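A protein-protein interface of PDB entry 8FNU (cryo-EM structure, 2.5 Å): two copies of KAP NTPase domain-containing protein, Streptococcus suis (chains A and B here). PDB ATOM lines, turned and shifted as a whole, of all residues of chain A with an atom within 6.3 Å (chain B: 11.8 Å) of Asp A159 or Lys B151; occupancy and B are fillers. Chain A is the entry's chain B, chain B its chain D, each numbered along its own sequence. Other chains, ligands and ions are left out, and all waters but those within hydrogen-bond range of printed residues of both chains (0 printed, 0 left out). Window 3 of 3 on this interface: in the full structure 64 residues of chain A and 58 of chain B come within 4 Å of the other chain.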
ATOM      1  N   ASN A 135     -25.674 -16.028  29.143  1.00  0.00           N
ATOM      2  CA  ASN A 135     -24.930 -15.079  28.321  1.00  0.00           C
ATOM      3  C   ASN A 135     -24.333 -15.734  27.097  1.00  0.00           C
ATOM      4  O   ASN A 135     -24.362 -15.158  26.009  1.00  0.00           O
ATOM      5  CB  ASN A 135     -23.785 -14.428  29.082  1.00  0.00           C
ATOM      6  CG  ASN A 135     -23.532 -13.006  28.628  1.00  0.00           C
ATOM      7  OD1 ASN A 135     -23.160 -12.152  29.443  1.00  0.00           O
ATOM      8  ND2 ASN A 135     -23.918 -12.699  27.394  1.00  0.00           N
ATOM      9  N   ALA A 136     -23.690 -16.886  27.273  1.00  0.00           N
ATOM     10  CA  ALA A 136     -23.069 -17.542  26.132  1.00  0.00           C
ATOM     11  C   ALA A 136     -24.112 -17.865  25.074  1.00  0.00           C
ATOM     12  O   ALA A 136     -23.874 -17.688  23.872  1.00  0.00           O
ATOM     13  CB  ALA A 136     -22.346 -18.804  26.590  1.00  0.00           C
ATOM     14  N   ALA A 138     -26.951 -16.251  24.566  1.00  0.00           N
ATOM     15  CA  ALA A 138     -27.344 -14.997  23.929  1.00  0.00           C
ATOM     16  C   ALA A 138     -26.285 -14.529  22.936  1.00  0.00           C
ATOM     17  O   ALA A 138     -26.614 -14.046  21.847  1.00  0.00           O
ATOM     18  CB  ALA A 138     -27.595 -13.925  24.988  1.00  0.00           C
ATOM     19  N   VAL A 139     -25.009 -14.662  23.300  1.00  0.00           N
ATOM     20  CA  VAL A 139     -23.921 -14.267  22.410  1.00  0.00           C
ATOM     21  C   VAL A 139     -23.967 -15.088  21.131  1.00  0.00           C
ATOM     22  O   VAL A 139     -23.824 -14.552  20.025  1.00  0.00           O
ATOM     23  CB  VAL A 139     -22.565 -14.419  23.128  1.00  0.00           C
ATOM     24  CG1 VAL A 139     -21.424 -14.477  22.121  1.00  0.00           C
ATOM     25  CG2 VAL A 139     -22.352 -13.282  24.113  1.00  0.00           C
ATOM     26  N   GLN A 143     -27.333 -11.648  20.193  1.00  0.00           N
ATOM     27  CA  GLN A 143     -28.271 -10.882  20.991  1.00  0.00           C
ATOM     28  C   GLN A 143     -27.608  -9.763  21.769  1.00  0.00           C
ATOM     29  O   GLN A 143     -28.211  -8.696  21.931  1.00  0.00           O
ATOM     30  CB  GLN A 143     -28.942 -11.804  22.004  1.00  0.00           C
ATOM     31  CG  GLN A 143     -30.350 -11.466  22.355  1.00  0.00           C
ATOM     32  CD  GLN A 143     -31.051 -12.662  22.943  1.00  0.00           C
ATOM     33  OE1 GLN A 143     -31.937 -13.254  22.304  1.00  0.00           O
ATOM     34  NE2 GLN A 143     -30.775 -12.937  24.212  1.00  0.00           N
ATOM     35  N   SER A 144     -26.403  -9.998  22.272  1.00  0.00           N
ATOM     36  CA  SER A 144     -25.767  -9.075  23.191  1.00  0.00           C
ATOM     37  C   SER A 144     -25.530  -7.727  22.517  1.00  0.00           C
ATOM     38  O   SER A 144     -25.637  -7.576  21.297  1.00  0.00           O
ATOM     39  CB  SER A 144     -24.456  -9.669  23.692  1.00  0.00           C
ATOM     40  OG  SER A 144     -23.552  -9.878  22.623  1.00  0.00           O
ATOM     41  N   ASP A 145     -25.205  -6.734  23.341  1.00  0.00           N
ATOM     42  CA  ASP A 145     -24.949  -5.392  22.844  1.00  0.00           C
ATOM     43  C   ASP A 145     -23.745  -5.337  21.917  1.00  0.00           C
ATOM     44  O   ASP A 145     -23.576  -4.341  21.205  1.00  0.00           O
ATOM     45  CB  ASP A 145     -24.739  -4.437  24.021  1.00  0.00           C
ATOM     46  CG  ASP A 145     -26.030  -3.783  24.472  1.00  0.00           C
ATOM     47  OD1 ASP A 145     -26.456  -4.037  25.617  1.00  0.00           O
ATOM     48  OD2 ASP A 145     -26.616  -3.010  23.684  1.00  0.00           O
ATOM     49  N   GLU A 155     -15.419  -4.191  28.100  1.00  0.00           N
ATOM     50  CA  GLU A 155     -15.852  -5.225  29.037  1.00  0.00           C
ATOM     51  C   GLU A 155     -16.873  -6.177  28.420  1.00  0.00           C
ATOM     52  O   GLU A 155     -17.008  -7.312  28.891  1.00  0.00           O
ATOM     53  CB  GLU A 155     -16.398  -4.602  30.325  1.00  0.00           C
ATOM     54  CG  GLU A 155     -17.725  -3.822  30.262  1.00  0.00           C
ATOM     55  CD  GLU A 155     -17.663  -2.529  29.457  1.00  0.00           C
ATOM     56  OE1 GLU A 155     -16.659  -2.290  28.754  1.00  0.00           O
ATOM     57  OE2 GLU A 155     -18.630  -1.745  29.528  1.00  0.00           O
ATOM     58  N   MET A 156     -17.588  -5.764  27.371  1.00  0.00           N
ATOM     59  CA  MET A 156     -18.463  -6.718  26.696  1.00  0.00           C
ATOM     60  C   MET A 156     -17.664  -7.837  26.042  1.00  0.00           C
ATOM     61  O   MET A 156     -18.229  -8.897  25.750  1.00  0.00           O
ATOM     62  CB  MET A 156     -19.333  -6.029  25.645  1.00  0.00           C
ATOM     63  CG  MET A 156     -18.572  -5.548  24.422  1.00  0.00           C
ATOM     64  SD  MET A 156     -19.554  -4.657  23.196  1.00  0.00           S
ATOM     65  CE  MET A 156     -20.717  -3.744  24.203  1.00  0.00           C
ATOM     66  N   LEU A 157     -16.368  -7.624  25.805  1.00  0.00           N
ATOM     67  CA  LEU A 157     -15.514  -8.703  25.330  1.00  0.00           C
ATOM     68  C   LEU A 157     -15.474  -9.861  26.316  1.00  0.00           C
ATOM     69  O   LEU A 157     -15.185 -10.995  25.915  1.00  0.00           O
ATOM     70  CB  LEU A 157     -14.100  -8.177  25.077  1.00  0.00           C
ATOM     71  CG  LEU A 157     -13.232  -8.940  24.075  1.00  0.00           C
ATOM     72  CD1 LEU A 157     -13.946  -9.117  22.744  1.00  0.00           C
ATOM     73  CD2 LEU A 157     -11.902  -8.229  23.881  1.00  0.00           C
ATOM     74  N   THR A 158     -15.753  -9.602  27.594  1.00  0.00           N
ATOM     75  CA  THR A 158     -15.898 -10.692  28.551  1.00  0.00           C
ATOM     76  C   THR A 158     -17.068 -11.591  28.169  1.00  0.00           C
ATOM     77  O   THR A 158     -16.962 -12.822  28.228  1.00  0.00           O
ATOM     78  CB  THR A 158     -16.089 -10.131  29.960  1.00  0.00           C
ATOM     79  OG1 THR A 158     -14.932  -9.375  30.338  1.00  0.00           O
ATOM     80  CG2 THR A 158     -16.308 -11.252  30.963  1.00  0.00           C
ATOM     81  N   ASP A 159     -18.188 -10.992  27.757  1.00  0.00           N
ATOM     82  CA  ASP A 159     -19.353 -11.784  27.382  1.00  0.00           C
ATOM     83  C   ASP A 159     -19.026 -12.733  26.239  1.00  0.00           C
ATOM     84  O   ASP A 159     -19.396 -13.913  26.274  1.00  0.00           O
ATOM     85  CB  ASP A 159     -20.512 -10.863  27.001  1.00  0.00           C
ATOM     86  CG  ASP A 159     -20.862  -9.881  28.100  1.00  0.00           C
ATOM     87  OD1 ASP A 159     -21.093 -10.326  29.245  1.00  0.00           O
ATOM     88  OD2 ASP A 159     -20.908  -8.665  27.822  1.00  0.00           O
ATOM     89  N   LEU A 160     -18.324 -12.242  25.215  1.00  0.00           N
ATOM     90  CA  LEU A 160     -17.886 -13.128  24.142  1.00  0.00           C
ATOM     91  C   LEU A 160     -17.085 -14.294  24.701  1.00  0.00           C
ATOM     92  O   LEU A 160     -17.259 -15.442  24.270  1.00  0.00           O
ATOM     93  CB  LEU A 160     -17.053 -12.352  23.122  1.00  0.00           C
ATOM     94  CG  LEU A 160     -17.739 -11.226  22.342  1.00  0.00           C
ATOM     95  CD1 LEU A 160     -16.944 -10.916  21.087  1.00  0.00           C
ATOM     96  CD2 LEU A 160     -19.176 -11.577  21.990  1.00  0.00           C
ATOM     97  N   SER A 161     -16.215 -14.025  25.677  1.00  0.00           N
ATOM     98  CA  SER A 161     -15.444 -15.101  26.288  1.00  0.00           C
ATOM     99  C   SER A 161     -16.365 -16.171  26.859  1.00  0.00           C
ATOM    100  O   SER A 161     -16.097 -17.370  26.720  1.00  0.00           O
ATOM    101  CB  SER A 161     -14.529 -14.540  27.375  1.00  0.00           C
ATOM    102  OG  SER A 161     -15.184 -14.508  28.630  1.00  0.00           O
ATOM    103  N   HIS A 162     -17.477 -15.755  27.473  1.00  0.00           N
ATOM    104  CA  HIS A 162     -18.404 -16.722  28.049  1.00  0.00           C
ATOM    105  C   HIS A 162     -18.854 -17.742  27.015  1.00  0.00           C
ATOM    106  O   HIS A 162     -19.159 -18.887  27.366  1.00  0.00           O
ATOM    107  CB  HIS A 162     -19.617 -16.005  28.642  1.00  0.00           C
ATOM    108  CG  HIS A 162     -19.321 -15.247  29.898  1.00  0.00           C
ATOM    109  ND1 HIS A 162     -20.058 -14.153  30.296  1.00  0.00           N
ATOM    110  CD2 HIS A 162     -18.371 -15.425  30.846  1.00  0.00           C
ATOM    111  CE1 HIS A 162     -19.574 -13.689  31.434  1.00  0.00           C
ATOM    112  NE2 HIS A 162     -18.549 -14.444  31.789  1.00  0.00           N
ATOM    113  N   ARG A 163     -18.903 -17.351  25.741  1.00  0.00           N
ATOM    114  CA  ARG A 163     -19.257 -18.289  24.686  1.00  0.00           C
ATOM    115  C   ARG A 163     -18.051 -19.033  24.133  1.00  0.00           C
ATOM    116  O   ARG A 163     -18.181 -20.198  23.744  1.00  0.00           O
ATOM    117  CB  ARG A 163     -19.974 -17.562  23.545  1.00  0.00           C
ATOM    118  CG  ARG A 163     -20.506 -18.477  22.440  1.00  0.00           C
ATOM    119  CD  ARG A 163     -21.349 -19.629  22.975  1.00  0.00           C
ATOM    120  NE  ARG A 163     -21.692 -20.594  21.938  1.00  0.00           N
ATOM    121  CZ  ARG A 163     -20.899 -21.579  21.541  1.00  0.00           C
ATOM    122  NH1 ARG A 163     -19.691 -21.747  22.054  1.00  0.00           N
ATOM    123  NH2 ARG A 163     -21.329 -22.420  20.605  1.00  0.00           N
ATOM    124  N   THR A 164     -16.881 -18.393  24.086  1.00  0.00           N
ATOM    125  CA  THR A 164     -15.684 -19.074  23.612  1.00  0.00           C
ATOM    126  C   THR A 164     -15.112 -20.026  24.651  1.00  0.00           C
ATOM    127  O   THR A 164     -14.256 -20.848  24.311  1.00  0.00           O
ATOM    128  CB  THR A 164     -14.612 -18.058  23.207  1.00  0.00           C
ATOM    129  OG1 THR A 164     -14.159 -17.343  24.361  1.00  0.00           O
ATOM    130  CG2 THR A 164     -15.161 -17.075  22.187  1.00  0.00           C
ATOM    131  N   SER B 144     -40.889 -13.839  23.945  1.00  0.00           N
ATOM    132  CA  SER B 144     -40.527 -13.347  25.259  1.00  0.00           C
ATOM    133  C   SER B 144     -39.258 -12.503  25.182  1.00  0.00           C
ATOM    134  O   SER B 144     -38.537 -12.491  24.180  1.00  0.00           O
ATOM    135  CB  SER B 144     -40.343 -14.519  26.216  1.00  0.00           C
ATOM    136  OG  SER B 144     -39.292 -15.364  25.785  1.00  0.00           O
ATOM    137  N   ASP B 145     -38.991 -11.786  26.271  1.00  0.00           N
ATOM    138  CA  ASP B 145     -37.816 -10.934  26.347  1.00  0.00           C
ATOM    139  C   ASP B 145     -36.520 -11.725  26.258  1.00  0.00           C
ATOM    140  O   ASP B 145     -35.462 -11.127  26.026  1.00  0.00           O
ATOM    141  CB  ASP B 145     -37.843 -10.130  27.647  1.00  0.00           C
ATOM    142  CG  ASP B 145     -38.530  -8.788  27.485  1.00  0.00           C
ATOM    143  OD1 ASP B 145     -39.588  -8.582  28.116  1.00  0.00           O
ATOM    144  OD2 ASP B 145     -38.011  -7.937  26.730  1.00  0.00           O
ATOM    145  N   TYR B 146     -36.576 -13.046  26.435  1.00  0.00           N
ATOM    146  CA  TYR B 146     -35.366 -13.857  26.387  1.00  0.00           C
ATOM    147  C   TYR B 146     -34.709 -13.795  25.014  1.00  0.00           C
ATOM    148  O   TYR B 146     -33.478 -13.804  24.905  1.00  0.00           O
ATOM    149  CB  TYR B 146     -35.699 -15.301  26.765  1.00  0.00           C
ATOM    150  CG  TYR B 146     -34.526 -16.246  26.668  1.00  0.00           C
ATOM    151  CD1 TYR B 146     -33.578 -16.304  27.677  1.00  0.00           C
ATOM    152  CD2 TYR B 146     -34.370 -17.082  25.573  1.00  0.00           C
ATOM    153  CE1 TYR B 146     -32.504 -17.166  27.598  1.00  0.00           C
ATOM    154  CE2 TYR B 146     -33.299 -17.947  25.484  1.00  0.00           C
ATOM    155  CZ  TYR B 146     -32.368 -17.984  26.499  1.00  0.00           C
ATOM    156  OH  TYR B 146     -31.299 -18.844  26.417  1.00  0.00           O
ATOM    157  N   PHE B 147     -35.512 -13.733  23.953  1.00  0.00           N
ATOM    158  CA  PHE B 147     -34.999 -13.721  22.589  1.00  0.00           C
ATOM    159  C   PHE B 147     -34.788 -12.316  22.040  1.00  0.00           C
ATOM    160  O   PHE B 147     -34.408 -12.177  20.873  1.00  0.00           O
ATOM    161  CB  PHE B 147     -35.952 -14.481  21.662  1.00  0.00           C
ATOM    162  CG  PHE B 147     -36.388 -15.813  22.196  1.00  0.00           C
ATOM    163  CD1 PHE B 147     -37.516 -15.917  22.991  1.00  0.00           C
ATOM    164  CD2 PHE B 147     -35.676 -16.961  21.900  1.00  0.00           C
ATOM    165  CE1 PHE B 147     -37.922 -17.140  23.482  1.00  0.00           C
ATOM    166  CE2 PHE B 147     -36.079 -18.186  22.389  1.00  0.00           C
ATOM    167  CZ  PHE B 147     -37.203 -18.276  23.180  1.00  0.00           C
ATOM    168  N   LYS B 148     -35.020 -11.275  22.842  1.00  0.00           N
ATOM    169  CA  LYS B 148     -34.925  -9.903  22.369  1.00  0.00           C
ATOM    170  C   LYS B 148     -34.097  -9.007  23.279  1.00  0.00           C
ATOM    171  O   LYS B 148     -34.039  -7.797  23.036  1.00  0.00           O
ATOM    172  CB  LYS B 148     -36.329  -9.298  22.210  1.00  0.00           C
ATOM    173  CG  LYS B 148     -37.140  -9.917  21.079  1.00  0.00           C
ATOM    174  CD  LYS B 148     -38.502  -9.258  20.905  1.00  0.00           C
ATOM    175  CE  LYS B 148     -39.345  -9.310  22.169  1.00  0.00           C
ATOM    176  NZ  LYS B 148     -40.669  -8.660  21.961  1.00  0.00           N
ATOM    177  N   GLN B 149     -33.458  -9.558  24.309  1.00  0.00           N
ATOM    178  CA  GLN B 149     -32.678  -8.791  25.269  1.00  0.00           C
ATOM    179  C   GLN B 149     -31.199  -9.154  25.155  1.00  0.00           C
ATOM    180  O   GLN B 149     -30.842 -10.332  25.068  1.00  0.00           O
ATOM    181  CB  GLN B 149     -33.189  -9.044  26.692  1.00  0.00           C
ATOM    182  CG  GLN B 149     -32.253  -8.592  27.798  1.00  0.00           C
ATOM    183  CD  GLN B 149     -32.893  -8.724  29.178  1.00  0.00           C
ATOM    184  OE1 GLN B 149     -32.460  -9.547  29.990  1.00  0.00           O
ATOM    185  NE2 GLN B 149     -33.947  -7.945  29.441  1.00  0.00           N
ATOM    186  N   SER B 150     -30.344  -8.128  25.160  1.00  0.00           N
ATOM    187  CA  SER B 150     -28.903  -8.340  25.022  1.00  0.00           C
ATOM    188  C   SER B 150     -28.328  -9.079  26.229  1.00  0.00           C
ATOM    189  O   SER B 150     -27.382  -9.865  26.103  1.00  0.00           O
ATOM    190  CB  SER B 150     -28.210  -6.988  24.854  1.00  0.00           C
ATOM    191  OG  SER B 150     -28.643  -6.324  23.682  1.00  0.00           O
ATOM    192  N   LYS B 151     -28.895  -8.819  27.399  1.00  0.00           N
ATOM    193  CA  LYS B 151     -28.396  -9.136  28.736  1.00  0.00           C
ATOM    194  C   LYS B 151     -29.383  -9.991  29.516  1.00  0.00           C
ATOM    195  O   LYS B 151     -30.082  -9.481  30.408  1.00  0.00           O
ATOM    196  CB  LYS B 151     -28.128  -7.781  29.412  1.00  0.00           C
ATOM    197  CG  LYS B 151     -26.681  -7.260  29.274  1.00  0.00           C
ATOM    198  CD  LYS B 151     -25.666  -8.155  30.031  1.00  0.00           C
ATOM    199  CE  LYS B 151     -25.229  -9.555  29.734  1.00  0.00           C
ATOM    200  NZ  LYS B 151     -23.935  -9.941  30.368  1.00  0.00           N
ATOM    201  N   PRO B 152     -29.455 -11.298  29.238  1.00  0.00           N
ATOM    202  CA  PRO B 152     -30.507 -12.123  29.844  1.00  0.00           C
ATOM    203  C   PRO B 152     -30.441 -12.106  31.364  1.00  0.00           C
ATOM    204  O   PRO B 152     -29.365 -12.098  31.964  1.00  0.00           O
ATOM    205  CB  PRO B 152     -30.229 -13.525  29.283  1.00  0.00           C
ATOM    206  CG  PRO B 152     -29.405 -13.307  28.062  1.00  0.00           C
ATOM    207  CD  PRO B 152     -28.580 -12.095  28.362  1.00  0.00           C
ATOM    208  N   GLU B 153     -31.614 -12.091  31.986  1.00  0.00           N
ATOM    209  CA  GLU B 153     -31.743 -12.169  33.435  1.00  0.00           C
ATOM    210  C   GLU B 153     -32.097 -13.589  33.833  1.00  0.00           C
ATOM    211  O   GLU B 153     -32.569 -14.385  33.022  1.00  0.00           O
ATOM    212  CB  GLU B 153     -32.797 -11.189  33.956  1.00  0.00           C
ATOM    213  CG  GLU B 153     -32.466  -9.741  33.727  1.00  0.00           C
ATOM    214  CD  GLU B 153     -33.640  -8.789  33.499  1.00  0.00           C
ATOM    215  OE1 GLU B 153     -33.493  -7.934  32.600  1.00  0.00           O
ATOM    216  OE2 GLU B 153     -34.640  -8.853  34.239  1.00  0.00           O
ATOM    217  N   ILE B 154     -31.875 -13.897  35.109  1.00  0.00           N
ATOM    218  CA  ILE B 154     -32.020 -15.276  35.562  1.00  0.00           C
ATOM    219  C   ILE B 154     -33.483 -15.708  35.565  1.00  0.00           C
ATOM    220  O   ILE B 154     -33.809 -16.837  35.180  1.00  0.00           O
ATOM    221  CB  ILE B 154     -31.368 -15.453  36.949  1.00  0.00           C
ATOM    222  CG1 ILE B 154     -31.063 -16.930  37.234  1.00  0.00           C
ATOM    223  CG2 ILE B 154     -32.242 -14.866  38.057  1.00  0.00           C
ATOM    224  CD1 ILE B 154     -30.224 -17.637  36.183  1.00  0.00           C
ATOM    225  N   GLU B 155     -34.388 -14.823  35.990  1.00  0.00           N
ATOM    226  CA  GLU B 155     -35.755 -15.264  36.253  1.00  0.00           C
ATOM    227  C   GLU B 155     -36.542 -15.513  34.968  1.00  0.00           C
ATOM    228  O   GLU B 155     -37.515 -16.273  34.989  1.00  0.00           O
ATOM    229  CB  GLU B 155     -36.488 -14.266  37.156  1.00  0.00           C
ATOM    230  CG  GLU B 155     -36.832 -12.876  36.591  1.00  0.00           C
ATOM    231  CD  GLU B 155     -35.623 -11.993  36.300  1.00  0.00           C
ATOM    232  OE1 GLU B 155     -34.478 -12.488  36.332  1.00  0.00           O
ATOM    233  OE2 GLU B 155     -35.824 -10.789  36.037  1.00  0.00           O
ATOM    234  N   MET B 156     -36.147 -14.909  33.844  1.00  0.00           N
ATOM    235  CA  MET B 156     -36.812 -15.254  32.591  1.00  0.00           C
ATOM    236  C   MET B 156     -36.563 -16.706  32.209  1.00  0.00           C
ATOM    237  O   MET B 156     -37.317 -17.262  31.404  1.00  0.00           O
ATOM    238  CB  MET B 156     -36.359 -14.340  31.452  1.00  0.00           C
ATOM    239  CG  MET B 156     -34.931 -14.573  30.994  1.00  0.00           C
ATOM    240  SD  MET B 156     -34.335 -13.458  29.705  1.00  0.00           S
ATOM    241  CE  MET B 156     -35.122 -11.907  30.124  1.00  0.00           C
ATOM    242  N   LEU B 157     -35.522 -17.329  32.767  1.00  0.00           N
ATOM    243  CA  LEU B 157     -35.319 -18.757  32.569  1.00  0.00           C
ATOM    244  C   LEU B 157     -36.494 -19.567  33.093  1.00  0.00           C
ATOM    245  O   LEU B 157     -36.709 -20.696  32.639  1.00  0.00           O
ATOM    246  CB  LEU B 157     -34.026 -19.200  33.256  1.00  0.00           C
ATOM    247  CG  LEU B 157     -33.337 -20.458  32.721  1.00  0.00           C
ATOM    248  CD1 LEU B 157     -33.103 -20.367  31.220  1.00  0.00           C
ATOM    249  CD2 LEU B 157     -32.029 -20.697  33.456  1.00  0.00           C
ATOM    250  N   ASP B 159     -39.593 -18.679  32.516  1.00  0.00           N
ATOM    251  CA  ASP B 159     -40.519 -18.680  31.389  1.00  0.00           C
ATOM    252  C   ASP B 159     -40.180 -19.790  30.404  1.00  0.00           C
ATOM    253  O   ASP B 159     -41.072 -20.510  29.938  1.00  0.00           O
ATOM    254  CB  ASP B 159     -40.500 -17.320  30.694  1.00  0.00           C
ATOM    255  CG  ASP B 159     -40.809 -16.177  31.640  1.00  0.00           C
ATOM    256  OD1 ASP B 159     -41.851 -16.238  32.326  1.00  0.00           O
ATOM    257  OD2 ASP B 159     -40.011 -15.219  31.697  1.00  0.00           O
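The side-chain amino group (NZ) of Lys B151 sits at hydrogen-bond distance from the side-chain amide oxygen (OD1) of Asn A135 (2.5 Å). The backbone carbonyl oxygen of Tyr B146 is in hydrogen-bond range of the side-chain amide nitrogen of Gln A143 (2.9 Å). The backbone carbonyl oxygen (O) of Phe B147 lies close to the side-chain amide oxygen (OE1) of Gln A143 (3.1 Å). O of Gln B149 lies within hydrogen-bond range of NE2 of Gln A143. O of Gln A143 lies within hydrogen-bond range of OG of Ser B150. The backbone NH of Asp A145 sits close to the side-chain hydroxyl of Ser B150, 3.5 Å away. OD1 of Asp A159 is in salt-bridge range of NZ of Lys B151, at 3.1 Å.
The side-chain amide oxygen of Asn A135 sits close to the side-chain carboxylate of Asp A159 (2.8 Å). The backbone carbonyl oxygen (O) of Ala A138 is in hydrogen-bond range of the backbone NH (N) of Gln A143. The side-chain amide oxygen (OE1) of Gln B149 sits close to the backbone carbonyl oxygen (O) of Lys B151 (2.4 Å). The side-chain amide nitrogen (NE2) of Gln B149 lies within hydrogen-bond range of the side-chain carboxylate (OE1) of Glu B153.
Among the printed residues, merely in contact across the chains: Ser A144 with Ser B150 (3.4 Å), Ala A138 with Pro B152 (3.6 Å) and Gln A143 with Lys B148 (3.7 Å).
Asp A159 touches one residue of chain B. Of chain A, only Asn A135 and Asp A159 come within 4 Å of Lys B151. Asn A135 touches just one residue of chain B: Lys B151 (2.5 Å). Of chain B, only Ser B150 (3.4 Å) comes within 4 Å of Ser A144. No residue of chain B comes within 4 Å of Glu A155. Thr A158 touches none of the printed residues of chain B. No residue of chain B comes within 4 Å of Leu A160. No residue of chain B comes within 4 Å of His A162. Of the printed residues of chain A, Tyr B146 touches Gln A143 (2.9 Å). Printed residues of chain A within 4 Å of Phe B147: Gln A143 (3.0 Å). Printed residues of chain A within 4 Å of Gln B149: Gln A143 (2.7 Å). The nearest residue of chain A that does not touch Lys B151 is Asp A145 (4.9 Å). The nearest printed residue of chain B that does not touch Asp A145 is Lys B151 (4.9 Å).
Hydrophobic or aromatic side chains of chain A within 4 Å of the printed part of chain B: Ala A138. Of the 15 printed residues of chain B, 7 touch a printed residue of chain A. Among the printed residues, 10 pairs touch across the chains.
Positions printed for both chains: 144, 145, 155, 156, 157 and 159. Of the 10 pairs that touch across the chains among the printed residues, none has its exchanged pair printed and touching as well.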
